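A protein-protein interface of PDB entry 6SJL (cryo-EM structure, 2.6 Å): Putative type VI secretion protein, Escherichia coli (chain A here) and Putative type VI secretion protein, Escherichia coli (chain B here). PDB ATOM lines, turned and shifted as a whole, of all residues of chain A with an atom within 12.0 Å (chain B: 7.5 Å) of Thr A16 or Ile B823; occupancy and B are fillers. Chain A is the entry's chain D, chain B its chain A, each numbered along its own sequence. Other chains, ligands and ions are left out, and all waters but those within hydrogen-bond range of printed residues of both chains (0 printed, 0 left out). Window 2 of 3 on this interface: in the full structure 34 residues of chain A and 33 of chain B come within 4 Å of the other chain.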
ATOM      1  N   ALA A  12      12.447  20.948   8.300  1.00  0.00           N
ATOM      2  CA  ALA A  12      13.069  21.315   7.040  1.00  0.00           C
ATOM      3  C   ALA A  12      13.618  22.731   7.061  1.00  0.00           C
ATOM      4  O   ALA A  12      13.785  23.337   5.998  1.00  0.00           O
ATOM      5  CB  ALA A  12      12.063  21.154   5.898  1.00  0.00           C
ATOM      6  N   THR A  13      13.884  23.276   8.243  1.00  0.00           N
ATOM      7  CA  THR A  13      14.378  24.634   8.383  1.00  0.00           C
ATOM      8  C   THR A  13      15.609  24.621   9.273  1.00  0.00           C
ATOM      9  O   THR A  13      15.648  23.906  10.278  1.00  0.00           O
ATOM     10  CB  THR A  13      13.313  25.562   8.982  1.00  0.00           C
ATOM     11  OG1 THR A  13      13.220  25.341  10.395  1.00  0.00           O
ATOM     12  CG2 THR A  13      11.951  25.308   8.339  1.00  0.00           C
ATOM     13  N   HIS A  14      16.607  25.416   8.901  1.00  0.00           N
ATOM     14  CA  HIS A  14      17.833  25.535   9.677  1.00  0.00           C
ATOM     15  C   HIS A  14      18.586  26.765   9.208  1.00  0.00           C
ATOM     16  O   HIS A  14      18.592  27.087   8.018  1.00  0.00           O
ATOM     17  CB  HIS A  14      18.712  24.285   9.547  1.00  0.00           C
ATOM     18  CG  HIS A  14      20.050  24.412  10.205  1.00  0.00           C
ATOM     19  ND1 HIS A  14      20.213  24.426  11.573  1.00  0.00           N
ATOM     20  CD2 HIS A  14      21.293  24.527   9.679  1.00  0.00           C
ATOM     21  CE1 HIS A  14      21.497  24.545  11.862  1.00  0.00           C
ATOM     22  NE2 HIS A  14      22.174  24.609  10.729  1.00  0.00           N
ATOM     23  N   LYS A  15      19.205  27.451  10.160  1.00  0.00           N
ATOM     24  CA  LYS A  15      19.967  28.662   9.909  1.00  0.00           C
ATOM     25  C   LYS A  15      21.452  28.372  10.088  1.00  0.00           C
ATOM     26  O   LYS A  15      21.841  27.360  10.676  1.00  0.00           O
ATOM     27  CB  LYS A  15      19.510  29.786  10.844  1.00  0.00           C
ATOM     28  CG  LYS A  15      20.019  31.173  10.482  1.00  0.00           C
ATOM     29  CD  LYS A  15      19.483  32.224  11.437  1.00  0.00           C
ATOM     30  CE  LYS A  15      17.991  32.469  11.224  1.00  0.00           C
ATOM     31  NZ  LYS A  15      17.699  33.099   9.910  1.00  0.00           N
ATOM     32  N   THR A  16      22.282  29.269   9.565  1.00  0.00           N
ATOM     33  CA  THR A  16      23.725  29.088   9.556  1.00  0.00           C
ATOM     34  C   THR A  16      24.394  30.112  10.460  1.00  0.00           C
ATOM     35  O   THR A  16      24.002  31.280  10.492  1.00  0.00           O
ATOM     36  CB  THR A  16      24.284  29.205   8.134  1.00  0.00           C
ATOM     37  OG1 THR A  16      23.677  28.208   7.305  1.00  0.00           O
ATOM     38  CG2 THR A  16      25.806  29.016   8.123  1.00  0.00           C
ATOM     39  N   SER A  17      25.398  29.657  11.198  1.00  0.00           N
ATOM     40  CA  SER A  17      26.272  30.519  11.981  1.00  0.00           C
ATOM     41  C   SER A  17      27.651  29.870  11.995  1.00  0.00           C
ATOM     42  O   SER A  17      27.926  28.951  11.217  1.00  0.00           O
ATOM     43  CB  SER A  17      25.700  30.747  13.391  1.00  0.00           C
ATOM     44  OG  SER A  17      25.778  29.570  14.177  1.00  0.00           O
ATOM     45  N   ILE A  18      28.522  30.336  12.890  1.00  0.00           N
ATOM     46  CA  ILE A  18      29.895  29.842  12.918  1.00  0.00           C
ATOM     47  C   ILE A  18      30.054  28.558  13.712  1.00  0.00           C
ATOM     48  O   ILE A  18      31.173  28.037  13.800  1.00  0.00           O
ATOM     49  CB  ILE A  18      30.834  30.929  13.476  1.00  0.00           C
ATOM     50  CG1 ILE A  18      30.498  31.224  14.934  1.00  0.00           C
ATOM     51  CG2 ILE A  18      30.715  32.200  12.653  1.00  0.00           C
ATOM     52  CD1 ILE A  18      31.533  32.086  15.626  1.00  0.00           C
ATOM     53  N   HIS A  19      28.975  28.026  14.295  1.00  0.00           N
ATOM     54  CA  HIS A  19      29.075  26.804  15.089  1.00  0.00           C
ATOM     55  C   HIS A  19      29.277  25.563  14.227  1.00  0.00           C
ATOM     56  O   HIS A  19      29.935  24.619  14.674  1.00  0.00           O
ATOM     57  CB  HIS A  19      27.823  26.640  15.953  1.00  0.00           C
ATOM     58  CG  HIS A  19      26.586  26.312  15.173  1.00  0.00           C
ATOM     59  ND1 HIS A  19      25.952  27.225  14.360  1.00  0.00           N
ATOM     60  CD2 HIS A  19      25.835  25.188  15.130  1.00  0.00           C
ATOM     61  CE1 HIS A  19      24.885  26.665  13.819  1.00  0.00           C
ATOM     62  NE2 HIS A  19      24.790  25.428  14.272  1.00  0.00           N
ATOM     63  N   ASN A  20      28.752  25.564  13.003  1.00  0.00           N
ATOM     64  CA  ASN A  20      28.936  24.492  12.024  1.00  0.00           C
ATOM     65  C   ASN A  20      28.464  23.141  12.565  1.00  0.00           C
ATOM     66  O   ASN A  20      29.216  22.169  12.633  1.00  0.00           O
ATOM     67  CB  ASN A  20      30.398  24.406  11.583  1.00  0.00           C
ATOM     68  CG  ASN A  20      30.954  25.738  11.126  1.00  0.00           C
ATOM     69  OD1 ASN A  20      31.921  26.236  11.696  1.00  0.00           O
ATOM     70  ND2 ASN A  20      30.332  26.337  10.121  1.00  0.00           N
ATOM     71  N   ASP A  21      27.195  23.090  12.948  1.00  0.00           N
ATOM     72  CA  ASP A  21      26.570  21.847  13.377  1.00  0.00           C
ATOM     73  C   ASP A  21      25.492  21.431  12.382  1.00  0.00           C
ATOM     74  O   ASP A  21      25.169  22.152  11.436  1.00  0.00           O
ATOM     75  CB  ASP A  21      25.981  21.987  14.785  1.00  0.00           C
ATOM     76  CG  ASP A  21      27.042  22.272  15.836  1.00  0.00           C
ATOM     77  OD1 ASP A  21      28.243  22.178  15.516  1.00  0.00           O
ATOM     78  OD2 ASP A  21      26.671  22.585  16.986  1.00  0.00           O
ATOM     79  N   TRP A  22      24.917  20.256  12.621  1.00  0.00           N
ATOM     80  CA  TRP A  22      23.938  19.649  11.724  1.00  0.00           C
ATOM     81  C   TRP A  22      22.619  19.528  12.478  1.00  0.00           C
ATOM     82  O   TRP A  22      22.545  18.816  13.486  1.00  0.00           O
ATOM     83  CB  TRP A  22      24.409  18.278  11.246  1.00  0.00           C
ATOM     84  CG  TRP A  22      25.874  18.142  10.953  1.00  0.00           C
ATOM     85  CD1 TRP A  22      26.887  18.070  11.860  1.00  0.00           C
ATOM     86  CD2 TRP A  22      26.482  18.014   9.665  1.00  0.00           C
ATOM     87  NE1 TRP A  22      28.092  17.930  11.218  1.00  0.00           N
ATOM     88  CE2 TRP A  22      27.870  17.891   9.868  1.00  0.00           C
ATOM     89  CE3 TRP A  22      25.989  18.003   8.358  1.00  0.00           C
ATOM     90  CZ2 TRP A  22      28.770  17.759   8.812  1.00  0.00           C
ATOM     91  CZ3 TRP A  22      26.882  17.878   7.315  1.00  0.00           C
ATOM     92  CH2 TRP A  22      28.257  17.754   7.546  1.00  0.00           C
ATOM     93  N   LYS A  23      21.576  20.218  11.999  1.00  0.00           N
ATOM     94  CA  LYS A  23      20.353  20.355  12.786  1.00  0.00           C
ATOM     95  C   LYS A  23      19.646  19.028  13.059  1.00  0.00           C
ATOM     96  O   LYS A  23      19.918  18.397  14.081  1.00  0.00           O
ATOM     97  CB  LYS A  23      19.403  21.312  12.047  1.00  0.00           C
ATOM     98  CG  LYS A  23      17.997  21.456  12.625  1.00  0.00           C
ATOM     99  CD  LYS A  23      17.938  22.169  13.956  1.00  0.00           C
ATOM    100  CE  LYS A  23      18.146  23.653  13.786  1.00  0.00           C
ATOM    101  NZ  LYS A  23      17.024  24.263  13.015  1.00  0.00           N
ATOM    102  N   VAL A  24      18.826  18.558  12.112  1.00  0.00           N
ATOM    103  CA  VAL A  24      18.079  17.295  12.143  1.00  0.00           C
ATOM    104  C   VAL A  24      17.388  17.106  10.800  1.00  0.00           C
ATOM    105  O   VAL A  24      17.073  18.083  10.116  1.00  0.00           O
ATOM    106  CB  VAL A  24      17.012  17.217  13.258  1.00  0.00           C
ATOM    107  CG1 VAL A  24      17.588  16.883  14.623  1.00  0.00           C
ATOM    108  CG2 VAL A  24      16.208  18.503  13.309  1.00  0.00           C
ATOM    109  N   GLY B 778      29.959  25.805   6.950  1.00  0.00           N
ATOM    110  CA  GLY B 778      29.572  24.581   7.628  1.00  0.00           C
ATOM    111  C   GLY B 778      28.141  24.627   8.121  1.00  0.00           C
ATOM    112  O   GLY B 778      27.556  25.700   8.266  1.00  0.00           O
ATOM    113  N   GLY B 779      27.583  23.453   8.392  1.00  0.00           N
ATOM    114  CA  GLY B 779      26.192  23.333   8.772  1.00  0.00           C
ATOM    115  C   GLY B 779      25.419  22.458   7.812  1.00  0.00           C
ATOM    116  O   GLY B 779      25.509  22.635   6.594  1.00  0.00           O
ATOM    117  N   GLY B 780      24.663  21.515   8.340  1.00  0.00           N
ATOM    118  CA  GLY B 780      23.942  20.566   7.516  1.00  0.00           C
ATOM    119  C   GLY B 780      22.823  19.895   8.274  1.00  0.00           C
ATOM    120  O   GLY B 780      22.208  20.491   9.161  1.00  0.00           O
ATOM    121  N   THR B 800      19.365  27.772   0.148  1.00  0.00           N
ATOM    122  CA  THR B 800      19.486  28.865   1.098  1.00  0.00           C
ATOM    123  C   THR B 800      18.371  29.883   0.874  1.00  0.00           C
ATOM    124  O   THR B 800      17.645  29.844  -0.124  1.00  0.00           O
ATOM    125  CB  THR B 800      20.842  29.552   0.974  1.00  0.00           C
ATOM    126  OG1 THR B 800      20.799  30.508  -0.091  1.00  0.00           O
ATOM    127  CG2 THR B 800      21.924  28.526   0.680  1.00  0.00           C
ATOM    128  N   ALA B 801      18.234  30.807   1.825  1.00  0.00           N
ATOM    129  CA  ALA B 801      17.284  31.897   1.656  1.00  0.00           C
ATOM    130  C   ALA B 801      17.937  33.041   0.895  1.00  0.00           C
ATOM    131  O   ALA B 801      17.828  34.206   1.289  1.00  0.00           O
ATOM    132  CB  ALA B 801      16.770  32.378   3.015  1.00  0.00           C
ATOM    133  N   GLU B 802      18.623  32.713  -0.198  1.00  0.00           N
ATOM    134  CA  GLU B 802      19.202  33.710  -1.092  1.00  0.00           C
ATOM    135  C   GLU B 802      19.024  33.395  -2.569  1.00  0.00           C
ATOM    136  O   GLU B 802      19.018  34.327  -3.378  1.00  0.00           O
ATOM    137  CB  GLU B 802      20.697  33.892  -0.801  1.00  0.00           C
ATOM    138  CG  GLU B 802      20.993  34.486   0.562  1.00  0.00           C
ATOM    139  CD  GLU B 802      22.472  34.643   0.818  1.00  0.00           C
ATOM    140  OE1 GLU B 802      23.273  34.183  -0.021  1.00  0.00           O
ATOM    141  OE2 GLU B 802      22.835  35.227   1.858  1.00  0.00           O
ATOM    142  N   VAL B 819      27.138  23.931   4.262  1.00  0.00           N
ATOM    143  CA  VAL B 819      26.800  25.204   3.643  1.00  0.00           C
ATOM    144  C   VAL B 819      27.799  26.238   4.128  1.00  0.00           C
ATOM    145  O   VAL B 819      28.336  26.134   5.235  1.00  0.00           O
ATOM    146  CB  VAL B 819      25.353  25.630   3.970  1.00  0.00           C
ATOM    147  CG1 VAL B 819      24.373  24.548   3.558  1.00  0.00           C
ATOM    148  CG2 VAL B 819      25.212  25.942   5.455  1.00  0.00           C
ATOM    149  N   ASN B 820      28.076  27.243   3.292  1.00  0.00           N
ATOM    150  CA  ASN B 820      29.029  28.258   3.725  1.00  0.00           C
ATOM    151  C   ASN B 820      28.606  29.672   3.336  1.00  0.00           C
ATOM    152  O   ASN B 820      29.398  30.608   3.489  1.00  0.00           O
ATOM    153  CB  ASN B 820      30.428  27.961   3.168  1.00  0.00           C
ATOM    154  CG  ASN B 820      31.528  28.671   3.943  1.00  0.00           C
ATOM    155  OD1 ASN B 820      31.266  29.370   4.923  1.00  0.00           O
ATOM    156  ND2 ASN B 820      32.765  28.492   3.507  1.00  0.00           N
ATOM    157  N   THR B 821      27.392  29.874   2.844  1.00  0.00           N
ATOM    158  CA  THR B 821      26.967  31.258   2.748  1.00  0.00           C
ATOM    159  C   THR B 821      26.643  31.763   4.151  1.00  0.00           C
ATOM    160  O   THR B 821      26.340  30.984   5.059  1.00  0.00           O
ATOM    161  CB  THR B 821      25.776  31.421   1.808  1.00  0.00           C
ATOM    162  OG1 THR B 821      24.576  31.034   2.482  1.00  0.00           O
ATOM    163  CG2 THR B 821      25.959  30.565   0.566  1.00  0.00           C
ATOM    164  N   SER B 822      26.714  33.085   4.319  1.00  0.00           N
ATOM    165  CA  SER B 822      26.975  33.653   5.637  1.00  0.00           C
ATOM    166  C   SER B 822      25.943  33.242   6.682  1.00  0.00           C
ATOM    167  O   SER B 822      26.262  32.447   7.571  1.00  0.00           O
ATOM    168  CB  SER B 822      27.052  35.179   5.540  1.00  0.00           C
ATOM    169  OG  SER B 822      25.944  35.715   4.837  1.00  0.00           O
ATOM    170  N   ILE B 823      24.705  33.717   6.565  1.00  0.00           N
ATOM    171  CA  ILE B 823      23.641  33.362   7.506  1.00  0.00           C
ATOM    172  C   ILE B 823      22.300  33.405   6.780  1.00  0.00           C
ATOM    173  O   ILE B 823      21.555  34.387   6.920  1.00  0.00           O
ATOM    174  CB  ILE B 823      23.606  34.291   8.736  1.00  0.00           C
ATOM    175  CG1 ILE B 823      24.921  34.289   9.516  1.00  0.00           C
ATOM    176  CG2 ILE B 823      22.500  33.873   9.702  1.00  0.00           C
ATOM    177  CD1 ILE B 823      25.806  35.489   9.226  1.00  0.00           C
ATOM    178  N   PRO B 824      21.975  32.420   5.948  1.00  0.00           N
ATOM    179  CA  PRO B 824      20.584  32.265   5.513  1.00  0.00           C
ATOM    180  C   PRO B 824      19.860  31.225   6.350  1.00  0.00           C
ATOM    181  O   PRO B 824      20.465  30.595   7.223  1.00  0.00           O
ATOM    182  CB  PRO B 824      20.728  31.824   4.056  1.00  0.00           C
ATOM    183  CG  PRO B 824      21.999  31.060   4.044  1.00  0.00           C
ATOM    184  CD  PRO B 824      22.853  31.484   5.231  1.00  0.00           C
ATOM    185  N   SER B 825      18.576  31.017   6.081  1.00  0.00           N
ATOM    186  CA  SER B 825      17.807  29.933   6.687  1.00  0.00           C
ATOM    187  C   SER B 825      17.606  28.873   5.603  1.00  0.00           C
ATOM    188  O   SER B 825      16.750  29.023   4.726  1.00  0.00           O
ATOM    189  CB  SER B 825      16.483  30.446   7.247  1.00  0.00           C
ATOM    190  OG  SER B 825      15.753  29.417   7.891  1.00  0.00           O
ATOM    191  N   VAL B 826      18.405  27.806   5.667  1.00  0.00           N
ATOM    192  CA  VAL B 826      18.430  26.785   4.625  1.00  0.00           C
ATOM    193  C   VAL B 826      17.251  25.833   4.788  1.00  0.00           C
ATOM    194  O   VAL B 826      16.728  25.630   5.891  1.00  0.00           O
ATOM    195  CB  VAL B 826      19.774  26.031   4.645  1.00  0.00           C
ATOM    196  CG1 VAL B 826      20.930  27.021   4.662  1.00  0.00           C
ATOM    197  CG2 VAL B 826      19.848  25.087   5.832  1.00  0.00           C
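Of the printed residues of chain B, Thr A16 touches Gly B778 (3.8 Å), Val B819 (3.3 Å), Thr B821 (3.7 Å), Ser B822 (3.5 Å), Ile B823 (3.1 Å), Pro B824 (3.2 Å) and Val B826 (3.99 Å).
Of the printed residues of chain B, Trp A22 touches Gly B780 (3.2 Å).
Of the printed residues of chain B, Lys A23 touches Gly B780.
Of chain A, only Thr A16 (3.8 Å) and Asn A20 (3.1 Å) come within 4 Å of Gly B778.
Of the printed residues of chain A, Val B819 touches Thr A16 (3.3 Å).
Thr B821 touches just one residue of chain A: Thr A16 (3.7 Å).
Of chain A, only Thr A16 (3.5 Å) comes within 4 Å of Ser B822.
Of chain A, only Lys A15 (3.3 Å) and Thr A16 (3.2 Å) come within 4 Å of Pro B824.
Of chain A, only His A14 and Lys A15 come within 4 Å of Ser B825.
The nearest printed residue of chain B that does not touch Thr A16 is Ser B825 (5.4 Å).
The nearest printed residue of chain A that does not touch Gly B780 is His A14 (4.2 Å).
Of the 13 printed residues of chain A, 9 touch a printed residue of chain B.
Printed residues of chain A that touch a printed residue of chain B: Ala A12, Thr A13, His A14, Lys A15, Thr A16, Asn A20, Asp A21, Trp A22 and Lys A23.
Of the 14 printed residues of chain B, 10 touch a printed residue of chain A.
Printed residues of chain B that touch a printed residue of chain A: Gly B778, Gly B779, Gly B780, Val B819, Thr B821, Ser B822, Ile B823, Pro B824, Ser B825 and Val B826.
Hydrophobic or aromatic side chains of chain B that line the printed part of chain A: Val B819, Ile B823, Pro B824 and Val B826.
The backbone NH (N) of Gly B778 sits close to the side-chain amide nitrogen (ND2) of Asn A20 (3.2 Å).
N of Gly B780 is in hydrogen-bond range of O of Asp A21.
N of Lys A23 sits at hydrogen-bond distance from O of Gly B780 (2.9 Å).
The backbone carbonyl oxygen of Pro B824 lies within hydrogen-bond range of the backbone NH of Thr A16, 3.2 Å away.
N of Val B826 lies within hydrogen-bond range of O of His A14 (2.5 Å).
Among the printed residues, pairs that only touch across the chains: Ala A12 with Val B826 (3.7 Å), Thr A13 with Val B826 (3.6 Å), His A14 with Ser B825 (3.2 Å), Lys A15 with Ile B823 (3.7 Å), Lys A15 with Pro B824 (3.3 Å), Lys A15 with Ser B825 (3.95 Å), Thr A16 with Gly B778 (3.8 Å), Thr A16 with Val B819 (3.3 Å), Thr A16 with Thr B821 (3.7 Å), Thr A16 with Ser B822 (3.5 Å), Thr A16 with Ile B823 (3.1 Å), Thr A16 with Val B826 (3.99 Å), Asp A21 with Gly B779 (3.1 Å) and Trp A22 with Gly B780 (3.2 Å).
The backbone NH of Val B819 is in hydrogen-bond range of the backbone carbonyl oxygen of Gly B779 (3.1 Å).
NZ of Lys A23 lies within hydrogen-bond range of O of Thr A13, 3.1 Å away.
The side-chain amide oxygen (OD1) of Asn A20 lies close to the backbone carbonyl oxygen (O) of Ile A18, at 2.9 Å.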
